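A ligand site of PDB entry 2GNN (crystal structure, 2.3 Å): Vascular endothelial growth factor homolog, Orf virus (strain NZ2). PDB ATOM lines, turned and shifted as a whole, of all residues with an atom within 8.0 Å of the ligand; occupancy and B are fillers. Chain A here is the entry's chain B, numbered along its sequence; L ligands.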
ATOM      1  N   LEU A  38     -22.726  -3.983 -26.494  1.00  0.00           N
ATOM      2  CA  LEU A  38     -21.788  -3.049 -27.125  1.00  0.00           C
ATOM      3  C   LEU A  38     -20.890  -2.429 -26.048  1.00  0.00           C
ATOM      4  O   LEU A  38     -21.114  -1.289 -25.603  1.00  0.00           O
ATOM      5  CB  LEU A  38     -22.545  -2.003 -27.921  1.00  0.00           C
ATOM      6  CG  LEU A  38     -23.260  -2.510 -29.195  1.00  0.00           C
ATOM      7  CD1 LEU A  38     -24.071  -1.377 -29.795  1.00  0.00           C
ATOM      8  CD2 LEU A  38     -22.267  -3.017 -30.196  1.00  0.00           C
ATOM      9  N   THR A  39     -19.909  -3.203 -25.611  1.00  0.00           N
ATOM     10  CA  THR A  39     -19.041  -2.887 -24.490  1.00  0.00           C
ATOM     11  C   THR A  39     -17.798  -2.182 -25.042  1.00  0.00           C
ATOM     12  O   THR A  39     -17.560  -2.212 -26.248  1.00  0.00           O
ATOM     13  CB  THR A  39     -18.523  -4.179 -23.879  1.00  0.00           C
ATOM     14  OG1 THR A  39     -18.042  -4.982 -24.941  1.00  0.00           O
ATOM     15  CG2 THR A  39     -19.580  -4.948 -23.109  1.00  0.00           C
ATOM     16  N   SER A  40     -16.998  -1.589 -24.150  1.00  0.00           N
ATOM     17  CA  SER A  40     -15.801  -0.798 -24.518  1.00  0.00           C
ATOM     18  C   SER A  40     -16.085   0.262 -25.588  1.00  0.00           C
ATOM     19  O   SER A  40     -15.322   0.426 -26.531  1.00  0.00           O
ATOM     20  CB  SER A  40     -14.658  -1.704 -24.986  1.00  0.00           C
ATOM     21  OG  SER A  40     -14.081  -2.363 -23.873  1.00  0.00           O
ATOM     22  N   GLN A  41     -17.204   0.956 -25.475  1.00  0.00           N
ATOM     23  CA  GLN A  41     -17.502   2.029 -26.422  1.00  0.00           C
ATOM     24  C   GLN A  41     -18.346   3.119 -25.772  1.00  0.00           C
ATOM     25  O   GLN A  41     -18.921   2.897 -24.700  1.00  0.00           O
ATOM     26  CB  GLN A  41     -18.137   1.518 -27.704  1.00  0.00           C
ATOM     27  CG  GLN A  41     -19.673   1.517 -27.722  1.00  0.00           C
ATOM     28  CD  GLN A  41     -20.209   1.321 -29.094  1.00  0.00           C
ATOM     29  OE1 GLN A  41     -20.223   0.211 -29.606  1.00  0.00           O
ATOM     30  NE2 GLN A  41     -20.653   2.417 -29.732  1.00  0.00           N
ATOM     31  N   ARG A  42     -18.396   4.292 -26.398  1.00  0.00           N
ATOM     32  CA  ARG A  42     -19.216   5.390 -25.911  1.00  0.00           C
ATOM     33  C   ARG A  42     -20.244   5.710 -26.944  1.00  0.00           C
ATOM     34  O   ARG A  42     -20.031   5.406 -28.114  1.00  0.00           O
ATOM     35  CB  ARG A  42     -18.358   6.623 -25.638  1.00  0.00           C
ATOM     36  CG  ARG A  42     -17.394   6.438 -24.485  1.00  0.00           C
ATOM     37  CD  ARG A  42     -17.355   7.650 -23.643  1.00  0.00           C
ATOM     38  NE  ARG A  42     -16.596   7.428 -22.434  1.00  0.00           N
ATOM     39  CZ  ARG A  42     -17.137   7.312 -21.224  1.00  0.00           C
ATOM     40  NH1 ARG A  42     -18.457   7.389 -21.083  1.00  0.00           N
ATOM     41  NH2 ARG A  42     -16.367   7.130 -20.164  1.00  0.00           N
ATOM     42  N   ALA A  79     -19.093   3.703 -32.416  1.00  0.00           N
ATOM     43  CA  ALA A  79     -17.832   3.163 -32.880  1.00  0.00           C
ATOM     44  C   ALA A  79     -17.995   2.464 -34.215  1.00  0.00           C
ATOM     45  O   ALA A  79     -19.026   1.856 -34.491  1.00  0.00           O
ATOM     46  CB  ALA A  79     -17.275   2.217 -31.844  1.00  0.00           C
ATOM     47  N   SER A  80     -16.972   2.580 -35.046  1.00  0.00           N
ATOM     48  CA  SER A  80     -16.858   1.819 -36.261  1.00  0.00           C
ATOM     49  C   SER A  80     -16.085   0.517 -36.007  1.00  0.00           C
ATOM     50  O   SER A  80     -15.635   0.217 -34.868  1.00  0.00           O
ATOM     51  CB  SER A  80     -16.095   2.642 -37.271  1.00  0.00           C
ATOM     52  OG  SER A  80     -14.770   2.781 -36.806  1.00  0.00           O
ATOM     53  N   GLY A  81     -15.893  -0.240 -37.079  1.00  0.00           N
ATOM     54  CA  GLY A  81     -15.170  -1.514 -37.050  1.00  0.00           C
ATOM     55  C   GLY A  81     -13.806  -1.427 -36.422  1.00  0.00           C
ATOM     56  O   GLY A  81     -13.380  -2.370 -35.737  1.00  0.00           O
ATOM     57  N   SER A  82     -13.131  -0.295 -36.616  1.00  0.00           N
ATOM     58  CA  SER A  82     -11.791  -0.075 -36.054  1.00  0.00           C
ATOM     59  C   SER A  82     -11.826   0.515 -34.670  1.00  0.00           C
ATOM     60  O   SER A  82     -10.767   0.733 -34.062  1.00  0.00           O
ATOM     61  CB  SER A  82     -10.967   0.840 -36.949  1.00  0.00           C
ATOM     62  OG  SER A  82     -11.565   2.118 -37.060  1.00  0.00           O
ATOM     63  N   GLY A  83     -13.032   0.766 -34.160  1.00  0.00           N
ATOM     64  CA  GLY A  83     -13.147   1.395 -32.825  1.00  0.00           C
ATOM     65  C   GLY A  83     -13.012   2.918 -32.910  1.00  0.00           C
ATOM     66  O   GLY A  83     -12.971   3.595 -31.899  1.00  0.00           O
ATOM     67  N   SER A  84     -12.961   3.446 -34.135  1.00  0.00           N
ATOM     68  CA  SER A  84     -12.963   4.875 -34.378  1.00  0.00           C
ATOM     69  C   SER A  84     -14.355   5.437 -34.122  1.00  0.00           C
ATOM     70  O   SER A  84     -15.290   4.685 -33.846  1.00  0.00           O
ATOM     71  CB  SER A  84     -12.555   5.139 -35.833  1.00  0.00           C
ATOM     72  OG  SER A  84     -11.228   4.687 -36.032  1.00  0.00           O
HETATM   73  C1  LIG L   1     -13.171  -2.229 -30.878  1.00  0.00           C
HETATM   74  C2  LIG L   1     -12.406  -2.804 -29.866  1.00  0.00           C
HETATM   75  C3  LIG L   1     -12.849  -2.733 -28.546  1.00  0.00           C
HETATM   76  C4  LIG L   1     -14.034  -2.049 -28.277  1.00  0.00           C
HETATM   77  C5  LIG L   1     -14.781  -1.437 -29.278  1.00  0.00           C
HETATM   78  C6  LIG L   1     -14.356  -1.544 -30.610  1.00  0.00           C
HETATM   79  C7  LIG L   1     -12.681  -2.345 -32.258  1.00  0.00           C
HETATM   80  N1  LIG L   1     -13.531  -2.652 -33.147  1.00  0.00           N
HETATM   81  N2  LIG L   1     -11.370  -2.188 -32.496  1.00  0.00           N
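Ser 40 touches the ligand.
Ser 80 touches the ligand (O to N1, 3.95 Å).
Gly 83 touches the ligand.
Five residues have an atom within 4 Å of the ligand: Ser 40, Ser 80, Gly 81, Ser 82 and Gly 83.
The side-chain hydroxyl (OG) of Ser 80 lies within hydrogen-bond range of the backbone NH (N) of Ser 84, 3.3 Å away.
The side-chain hydroxyl of Ser 80 lies within hydrogen-bond range of the side-chain hydroxyl of Ser 82 (3.3 Å).
OG of Ser 82 lies within hydrogen-bond range of OG of Ser 84, 2.8 Å away.
A nitrogen (N1) of the ligand sits at hydrogen-bond distance from the backbone carbonyl oxygen of Gly 81 (2.6 Å).
O of Ser 82 lies within hydrogen-bond range of N2 of the ligand (3.4 Å).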
